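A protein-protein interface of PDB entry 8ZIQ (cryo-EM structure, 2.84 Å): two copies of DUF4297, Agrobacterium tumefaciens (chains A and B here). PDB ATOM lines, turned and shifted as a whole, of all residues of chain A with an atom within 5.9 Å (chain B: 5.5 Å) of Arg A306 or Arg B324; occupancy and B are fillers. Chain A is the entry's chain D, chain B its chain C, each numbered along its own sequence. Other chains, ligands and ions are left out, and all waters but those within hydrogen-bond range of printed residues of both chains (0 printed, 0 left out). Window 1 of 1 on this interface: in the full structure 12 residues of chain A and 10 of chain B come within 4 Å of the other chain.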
ATOM      1  N   LEU A 300     -14.471  -9.620  30.484  1.00  0.00           N
ATOM      2  CA  LEU A 300     -13.049  -9.327  30.400  1.00  0.00           C
ATOM      3  C   LEU A 300     -12.715  -8.047  31.146  1.00  0.00           C
ATOM      4  O   LEU A 300     -11.664  -7.951  31.787  1.00  0.00           O
ATOM      5  CB  LEU A 300     -12.621  -9.239  28.945  1.00  0.00           C
ATOM      6  CG  LEU A 300     -12.336 -10.580  28.285  1.00  0.00           C
ATOM      7  CD1 LEU A 300     -12.305 -10.448  26.815  1.00  0.00           C
ATOM      8  CD2 LEU A 300     -11.030 -11.123  28.751  1.00  0.00           C
ATOM      9  N   TYR A 301     -13.594  -7.046  31.071  1.00  0.00           N
ATOM     10  CA  TYR A 301     -13.390  -5.842  31.865  1.00  0.00           C
ATOM     11  C   TYR A 301     -13.431  -6.155  33.349  1.00  0.00           C
ATOM     12  O   TYR A 301     -12.631  -5.628  34.126  1.00  0.00           O
ATOM     13  CB  TYR A 301     -14.460  -4.804  31.556  1.00  0.00           C
ATOM     14  CG  TYR A 301     -14.358  -3.576  32.419  1.00  0.00           C
ATOM     15  CD1 TYR A 301     -15.376  -3.226  33.279  1.00  0.00           C
ATOM     16  CD2 TYR A 301     -13.261  -2.747  32.347  1.00  0.00           C
ATOM     17  CE1 TYR A 301     -15.287  -2.114  34.066  1.00  0.00           C
ATOM     18  CE2 TYR A 301     -13.167  -1.629  33.130  1.00  0.00           C
ATOM     19  CZ  TYR A 301     -14.187  -1.313  33.982  1.00  0.00           C
ATOM     20  OH  TYR A 301     -14.099  -0.192  34.772  1.00  0.00           O
ATOM     21  N   GLY A 304     -10.109  -7.496  34.405  1.00  0.00           N
ATOM     22  CA  GLY A 304      -9.005  -6.565  34.458  1.00  0.00           C
ATOM     23  C   GLY A 304      -8.449  -6.147  33.122  1.00  0.00           C
ATOM     24  O   GLY A 304      -7.614  -5.237  33.084  1.00  0.00           O
ATOM     25  N   LEU A 305      -8.863  -6.771  32.030  1.00  0.00           N
ATOM     26  CA  LEU A 305      -8.298  -6.457  30.733  1.00  0.00           C
ATOM     27  C   LEU A 305      -9.097  -5.379  30.014  1.00  0.00           C
ATOM     28  O   LEU A 305     -10.197  -5.003  30.417  1.00  0.00           O
ATOM     29  CB  LEU A 305      -8.243  -7.711  29.878  1.00  0.00           C
ATOM     30  CG  LEU A 305      -7.447  -8.881  30.433  1.00  0.00           C
ATOM     31  CD1 LEU A 305      -7.305  -9.914  29.382  1.00  0.00           C
ATOM     32  CD2 LEU A 305      -6.093  -8.452  30.921  1.00  0.00           C
ATOM     33  N   ARG A 306      -8.518  -4.885  28.928  1.00  0.00           N
ATOM     34  CA  ARG A 306      -9.171  -3.959  28.025  1.00  0.00           C
ATOM     35  C   ARG A 306      -9.038  -4.489  26.607  1.00  0.00           C
ATOM     36  O   ARG A 306      -8.196  -5.340  26.320  1.00  0.00           O
ATOM     37  CB  ARG A 306      -8.582  -2.557  28.137  1.00  0.00           C
ATOM     38  CG  ARG A 306      -8.911  -1.830  29.425  1.00  0.00           C
ATOM     39  CD  ARG A 306      -8.331  -0.438  29.406  1.00  0.00           C
ATOM     40  NE  ARG A 306      -8.413   0.229  30.699  1.00  0.00           N
ATOM     41  CZ  ARG A 306      -9.454   0.948  31.100  1.00  0.00           C
ATOM     42  NH1 ARG A 306     -10.504   1.090  30.309  1.00  0.00           N
ATOM     43  NH2 ARG A 306      -9.445   1.525  32.294  1.00  0.00           N
ATOM     44  N   CYS A 307      -9.862  -3.957  25.711  1.00  0.00           N
ATOM     45  CA  CYS A 307     -10.018  -4.517  24.380  1.00  0.00           C
ATOM     46  C   CYS A 307     -10.199  -3.403  23.365  1.00  0.00           C
ATOM     47  O   CYS A 307     -10.431  -2.243  23.714  1.00  0.00           O
ATOM     48  CB  CYS A 307     -11.212  -5.467  24.312  1.00  0.00           C
ATOM     49  SG  CYS A 307     -11.003  -7.047  25.128  1.00  0.00           S
ATOM     50  N   GLU A 308     -10.095  -3.769  22.090  1.00  0.00           N
ATOM     51  CA  GLU A 308     -10.191  -2.826  20.981  1.00  0.00           C
ATOM     52  C   GLU A 308     -11.173  -3.382  19.957  1.00  0.00           C
ATOM     53  O   GLU A 308     -10.789  -4.091  19.025  1.00  0.00           O
ATOM     54  CB  GLU A 308      -8.844  -2.570  20.369  1.00  0.00           C
ATOM     55  CG  GLU A 308      -8.902  -1.770  19.098  1.00  0.00           C
ATOM     56  CD  GLU A 308      -9.630  -0.454  19.273  1.00  0.00           C
ATOM     57  OE1 GLU A 308      -9.242   0.330  20.164  1.00  0.00           O
ATOM     58  OE2 GLU A 308     -10.595  -0.201  18.521  1.00  0.00           O
ATOM     59  N   ARG A 334       2.511   1.050  31.179  1.00  0.00           N
ATOM     60  CA  ARG A 334       1.117   1.262  30.855  1.00  0.00           C
ATOM     61  C   ARG A 334       0.875   0.801  29.433  1.00  0.00           C
ATOM     62  O   ARG A 334       1.784   0.760  28.604  1.00  0.00           O
ATOM     63  CB  ARG A 334       0.708   2.714  31.030  1.00  0.00           C
ATOM     64  CG  ARG A 334       0.350   3.061  32.446  1.00  0.00           C
ATOM     65  CD  ARG A 334      -0.893   3.901  32.468  1.00  0.00           C
ATOM     66  NE  ARG A 334      -2.051   3.134  32.044  1.00  0.00           N
ATOM     67  CZ  ARG A 334      -3.280   3.627  31.950  1.00  0.00           C
ATOM     68  NH1 ARG A 334      -3.511   4.894  32.252  1.00  0.00           N
ATOM     69  NH2 ARG A 334      -4.272   2.853  31.542  1.00  0.00           N
ATOM     70  N   MET A 335      -0.375   0.458  29.160  1.00  0.00           N
ATOM     71  CA  MET A 335      -0.754  -0.092  27.873  1.00  0.00           C
ATOM     72  C   MET A 335      -2.185   0.312  27.580  1.00  0.00           C
ATOM     73  O   MET A 335      -3.081   0.076  28.395  1.00  0.00           O
ATOM     74  CB  MET A 335      -0.607  -1.607  27.889  1.00  0.00           C
ATOM     75  CG  MET A 335      -0.258  -2.221  26.574  1.00  0.00           C
ATOM     76  SD  MET A 335       0.499  -3.829  26.777  1.00  0.00           S
ATOM     77  CE  MET A 335       0.783  -4.220  25.072  1.00  0.00           C
ATOM     78  N   GLU A 336      -2.388   0.917  26.417  1.00  0.00           N
ATOM     79  CA  GLU A 336      -3.707   1.412  26.061  1.00  0.00           C
ATOM     80  C   GLU A 336      -4.689   0.267  25.876  1.00  0.00           C
ATOM     81  O   GLU A 336      -5.837   0.352  26.321  1.00  0.00           O
ATOM     82  CB  GLU A 336      -3.615   2.268  24.805  1.00  0.00           C
ATOM     83  CG  GLU A 336      -4.931   2.598  24.171  1.00  0.00           C
ATOM     84  CD  GLU A 336      -4.798   3.590  23.049  1.00  0.00           C
ATOM     85  OE1 GLU A 336      -5.521   3.451  22.045  1.00  0.00           O
ATOM     86  OE2 GLU A 336      -3.972   4.516  23.166  1.00  0.00           O
ATOM     87  N   PHE A 337      -4.263  -0.807  25.222  1.00  0.00           N
ATOM     88  CA  PHE A 337      -5.073  -2.007  25.165  1.00  0.00           C
ATOM     89  C   PHE A 337      -4.171  -3.212  24.984  1.00  0.00           C
ATOM     90  O   PHE A 337      -3.081  -3.114  24.422  1.00  0.00           O
ATOM     91  CB  PHE A 337      -6.136  -1.916  24.075  1.00  0.00           C
ATOM     92  CG  PHE A 337      -5.606  -1.750  22.698  1.00  0.00           C
ATOM     93  CD1 PHE A 337      -5.803  -0.576  22.029  1.00  0.00           C
ATOM     94  CD2 PHE A 337      -4.983  -2.780  22.042  1.00  0.00           C
ATOM     95  CE1 PHE A 337      -5.353  -0.415  20.770  1.00  0.00           C
ATOM     96  CE2 PHE A 337      -4.530  -2.608  20.774  1.00  0.00           C
ATOM     97  CZ  PHE A 337      -4.727  -1.427  20.142  1.00  0.00           C
ATOM     98  N   SER A 338      -4.647  -4.349  25.475  1.00  0.00           N
ATOM     99  CA  SER A 338      -3.909  -5.602  25.472  1.00  0.00           C
ATOM    100  C   SER A 338      -4.316  -6.542  24.350  1.00  0.00           C
ATOM    101  O   SER A 338      -3.452  -7.185  23.754  1.00  0.00           O
ATOM    102  CB  SER A 338      -4.096  -6.302  26.811  1.00  0.00           C
ATOM    103  OG  SER A 338      -3.193  -5.810  27.777  1.00  0.00           O
ATOM    104  N   LEU A 339      -5.604  -6.671  24.069  1.00  0.00           N
ATOM    105  CA  LEU A 339      -6.085  -7.587  23.052  1.00  0.00           C
ATOM    106  C   LEU A 339      -7.037  -6.909  22.078  1.00  0.00           C
ATOM    107  O   LEU A 339      -7.679  -5.907  22.393  1.00  0.00           O
ATOM    108  CB  LEU A 339      -6.755  -8.802  23.666  1.00  0.00           C
ATOM    109  CG  LEU A 339      -8.095  -8.666  24.349  1.00  0.00           C
ATOM    110  CD1 LEU A 339      -8.743  -9.982  24.374  1.00  0.00           C
ATOM    111  CD2 LEU A 339      -7.872  -8.203  25.761  1.00  0.00           C
ATOM    112  N   GLU B 308     -14.859   9.469  24.747  1.00  0.00           N
ATOM    113  CA  GLU B 308     -14.985   8.493  25.825  1.00  0.00           C
ATOM    114  C   GLU B 308     -16.461   8.318  26.173  1.00  0.00           C
ATOM    115  O   GLU B 308     -17.040   9.137  26.889  1.00  0.00           O
ATOM    116  CB  GLU B 308     -14.187   8.930  27.041  1.00  0.00           C
ATOM    117  CG  GLU B 308     -14.397   8.077  28.249  1.00  0.00           C
ATOM    118  CD  GLU B 308     -14.036   6.629  28.011  1.00  0.00           C
ATOM    119  OE1 GLU B 308     -13.176   6.363  27.145  1.00  0.00           O
ATOM    120  OE2 GLU B 308     -14.614   5.753  28.689  1.00  0.00           O
ATOM    121  N   LYS B 320     -16.876   4.763  36.454  1.00  0.00           N
ATOM    122  CA  LYS B 320     -15.440   4.912  36.624  1.00  0.00           C
ATOM    123  C   LYS B 320     -14.769   5.206  35.294  1.00  0.00           C
ATOM    124  O   LYS B 320     -13.821   5.997  35.232  1.00  0.00           O
ATOM    125  CB  LYS B 320     -14.857   3.659  37.263  1.00  0.00           C
ATOM    126  CG  LYS B 320     -15.269   3.463  38.702  1.00  0.00           C
ATOM    127  CD  LYS B 320     -14.864   2.096  39.227  1.00  0.00           C
ATOM    128  CE  LYS B 320     -13.361   1.989  39.417  1.00  0.00           C
ATOM    129  NZ  LYS B 320     -12.973   0.693  40.041  1.00  0.00           N
ATOM    130  N   GLU B 321     -15.241   4.580  34.218  1.00  0.00           N
ATOM    131  CA  GLU B 321     -14.574   4.721  32.934  1.00  0.00           C
ATOM    132  C   GLU B 321     -14.838   6.083  32.310  1.00  0.00           C
ATOM    133  O   GLU B 321     -14.020   6.571  31.523  1.00  0.00           O
ATOM    134  CB  GLU B 321     -15.013   3.614  31.996  1.00  0.00           C
ATOM    135  CG  GLU B 321     -14.430   2.284  32.344  1.00  0.00           C
ATOM    136  CD  GLU B 321     -12.966   2.184  32.001  1.00  0.00           C
ATOM    137  OE1 GLU B 321     -12.445   3.092  31.322  1.00  0.00           O
ATOM    138  OE2 GLU B 321     -12.326   1.192  32.413  1.00  0.00           O
ATOM    139  N   LEU B 322     -15.968   6.706  32.632  1.00  0.00           N
ATOM    140  CA  LEU B 322     -16.318   7.972  32.005  1.00  0.00           C
ATOM    141  C   LEU B 322     -15.455   9.109  32.519  1.00  0.00           C
ATOM    142  O   LEU B 322     -15.263  10.104  31.813  1.00  0.00           O
ATOM    143  CB  LEU B 322     -17.782   8.294  32.240  1.00  0.00           C
ATOM    144  CG  LEU B 322     -18.406   9.380  31.378  1.00  0.00           C
ATOM    145  CD1 LEU B 322     -18.312   9.115  29.926  1.00  0.00           C
ATOM    146  CD2 LEU B 322     -19.814   9.549  31.747  1.00  0.00           C
ATOM    147  N   PHE B 323     -14.930   8.988  33.734  1.00  0.00           N
ATOM    148  CA  PHE B 323     -14.284  10.098  34.414  1.00  0.00           C
ATOM    149  C   PHE B 323     -12.802   9.860  34.646  1.00  0.00           C
ATOM    150  O   PHE B 323     -12.169  10.630  35.375  1.00  0.00           O
ATOM    151  CB  PHE B 323     -14.960  10.392  35.750  1.00  0.00           C
ATOM    152  CG  PHE B 323     -16.380  10.823  35.634  1.00  0.00           C
ATOM    153  CD1 PHE B 323     -16.726  11.909  34.871  1.00  0.00           C
ATOM    154  CD2 PHE B 323     -17.363  10.183  36.341  1.00  0.00           C
ATOM    155  CE1 PHE B 323     -18.027  12.305  34.781  1.00  0.00           C
ATOM    156  CE2 PHE B 323     -18.656  10.586  36.252  1.00  0.00           C
ATOM    157  CZ  PHE B 323     -18.986  11.643  35.478  1.00  0.00           C
ATOM    158  N   ARG B 324     -12.232   8.819  34.056  1.00  0.00           N
ATOM    159  CA  ARG B 324     -10.833   8.519  34.265  1.00  0.00           C
ATOM    160  C   ARG B 324      -9.949   9.501  33.509  1.00  0.00           C
ATOM    161  O   ARG B 324     -10.413  10.327  32.720  1.00  0.00           O
ATOM    162  CB  ARG B 324     -10.540   7.088  33.845  1.00  0.00           C
ATOM    163  CG  ARG B 324     -10.811   6.803  32.419  1.00  0.00           C
ATOM    164  CD  ARG B 324     -10.382   5.422  32.071  1.00  0.00           C
ATOM    165  NE  ARG B 324     -10.747   5.061  30.711  1.00  0.00           N
ATOM    166  CZ  ARG B 324      -9.946   5.154  29.662  1.00  0.00           C
ATOM    167  NH1 ARG B 324      -8.699   5.571  29.793  1.00  0.00           N
ATOM    168  NH2 ARG B 324     -10.397   4.798  28.474  1.00  0.00           N
ATOM    169  N   ARG B 325      -8.655   9.394  33.760  1.00  0.00           N
ATOM    170  CA  ARG B 325      -7.632  10.243  33.186  1.00  0.00           C
ATOM    171  C   ARG B 325      -6.981   9.570  31.993  1.00  0.00           C
ATOM    172  O   ARG B 325      -6.699   8.368  32.035  1.00  0.00           O
ATOM    173  CB  ARG B 325      -6.564  10.579  34.220  1.00  0.00           C
ATOM    174  CG  ARG B 325      -6.989  11.608  35.232  1.00  0.00           C
ATOM    175  CD  ARG B 325      -5.833  11.990  36.135  1.00  0.00           C
ATOM    176  NE  ARG B 325      -6.094  13.220  36.876  1.00  0.00           N
ATOM    177  CZ  ARG B 325      -5.356  13.657  37.892  1.00  0.00           C
ATOM    178  NH1 ARG B 325      -4.300  12.965  38.299  1.00  0.00           N
ATOM    179  NH2 ARG B 325      -5.673  14.790  38.505  1.00  0.00           N
ATOM    180  N   PRO B 326      -6.731  10.313  30.922  1.00  0.00           N
ATOM    181  CA  PRO B 326      -6.113   9.733  29.736  1.00  0.00           C
ATOM    182  C   PRO B 326      -4.597   9.699  29.785  1.00  0.00           C
ATOM    183  O   PRO B 326      -3.946  10.395  30.564  1.00  0.00           O
ATOM    184  CB  PRO B 326      -6.577  10.685  28.634  1.00  0.00           C
ATOM    185  CG  PRO B 326      -6.685  11.937  29.297  1.00  0.00           C
ATOM    186  CD  PRO B 326      -7.146  11.694  30.668  1.00  0.00           C
ATOM    187  N   GLU B 336      -5.215  10.060  24.275  1.00  0.00           N
ATOM    188  CA  GLU B 336      -6.089   8.903  24.137  1.00  0.00           C
ATOM    189  C   GLU B 336      -7.494   9.318  23.740  1.00  0.00           C
ATOM    190  O   GLU B 336      -8.094   8.736  22.830  1.00  0.00           O
ATOM    191  CB  GLU B 336      -6.115   8.124  25.442  1.00  0.00           C
ATOM    192  CG  GLU B 336      -6.863   6.826  25.394  1.00  0.00           C
ATOM    193  CD  GLU B 336      -6.454   5.891  26.504  1.00  0.00           C
ATOM    194  OE1 GLU B 336      -6.832   6.151  27.664  1.00  0.00           O
ATOM    195  OE2 GLU B 336      -5.751   4.900  26.224  1.00  0.00           O
ATOM    196  N   PHE B 337      -8.037  10.328  24.409  1.00  0.00           N
ATOM    197  CA  PHE B 337      -9.284  10.935  23.991  1.00  0.00           C
ATOM    198  C   PHE B 337      -9.268  12.413  24.328  1.00  0.00           C
ATOM    199  O   PHE B 337      -8.606  12.845  25.273  1.00  0.00           O
ATOM    200  CB  PHE B 337     -10.488  10.246  24.629  1.00  0.00           C
ATOM    201  CG  PHE B 337     -10.498  10.289  26.117  1.00  0.00           C
ATOM    202  CD1 PHE B 337      -9.953   9.267  26.844  1.00  0.00           C
ATOM    203  CD2 PHE B 337     -11.073  11.338  26.788  1.00  0.00           C
ATOM    204  CE1 PHE B 337      -9.968   9.296  28.196  1.00  0.00           C
ATOM    205  CE2 PHE B 337     -11.083  11.362  28.147  1.00  0.00           C
ATOM    206  CZ  PHE B 337     -10.526  10.338  28.847  1.00  0.00           C
ATOM    207  N   ARG B 340     -15.516  13.909  26.171  1.00  0.00           N
ATOM    208  CA  ARG B 340     -16.415  12.943  26.777  1.00  0.00           C
ATOM    209  C   ARG B 340     -17.832  13.242  26.319  1.00  0.00           C
ATOM    210  O   ARG B 340     -18.251  14.401  26.297  1.00  0.00           O
ATOM    211  CB  ARG B 340     -16.344  12.993  28.274  1.00  0.00           C
ATOM    212  CG  ARG B 340     -14.969  12.893  28.823  1.00  0.00           C
ATOM    213  CD  ARG B 340     -15.009  12.819  30.303  1.00  0.00           C
ATOM    214  NE  ARG B 340     -13.900  12.067  30.870  1.00  0.00           N
ATOM    215  CZ  ARG B 340     -12.891  12.606  31.536  1.00  0.00           C
ATOM    216  NH1 ARG B 340     -12.830  13.894  31.729  1.00  0.00           N
ATOM    217  NH2 ARG B 340     -11.927  11.856  32.011  1.00  0.00           N
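The guanidinium group (NH1) of Arg A306 lies within salt-bridge range of the side-chain carboxylate (OE2) of Glu B321, 2.8 Å away.
The side-chain carboxylate (OE2) of Glu B321 sits close to the side-chain hydroxyl (OH) of Tyr A301, at 3.3 Å.
The side-chain carboxylate of Glu B321 is in salt-bridge range of the guanidinium group of Arg B324, at 2.7 Å.
NH2 of Arg B324 is in salt-bridge range of OE1 of Glu B308 (3.5 Å).
The guanidinium group (NH1) of Arg B324 lies within salt-bridge range of the side-chain carboxylate (OE1) of Glu B336 (2.9 Å).
Arg B324 touches Arg A306 (NE to NH1, 3.999 Å).
OE2 of Glu B336 touches CG of Glu A336 (3.2 Å).
Of the printed residues of chain B, Arg A306 touches Glu B321 and Arg B324.
Of the printed residues of chain A, Arg B324 touches Arg A306.
Of the printed residues of chain B, Glu A336 touches Glu B336.
Printed residues of chain A within 4 Å of Glu B321: Tyr A301 and Arg A306.
Of the printed residues of chain A, Glu B336 touches Glu A336 (3.2 Å).
Leu A339 touches none of the printed residues of chain B.
The nearest printed residue of chain B that does not touch Glu A336 is Arg B324 (6.7 Å).
Of the 13 printed residues of chain A, 3 touch a printed residue of chain B.
Hydrophobic or aromatic side chains of chain A that line the printed part of chain B: Tyr A301.
Among the printed residues, 4 pairs touch across the chains.
Glu A336 touches its own counterpart, Glu B336.
Of the 4 pairs that touch across the chains among the printed residues, 1 has its exchanged pair printed and touching as well.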
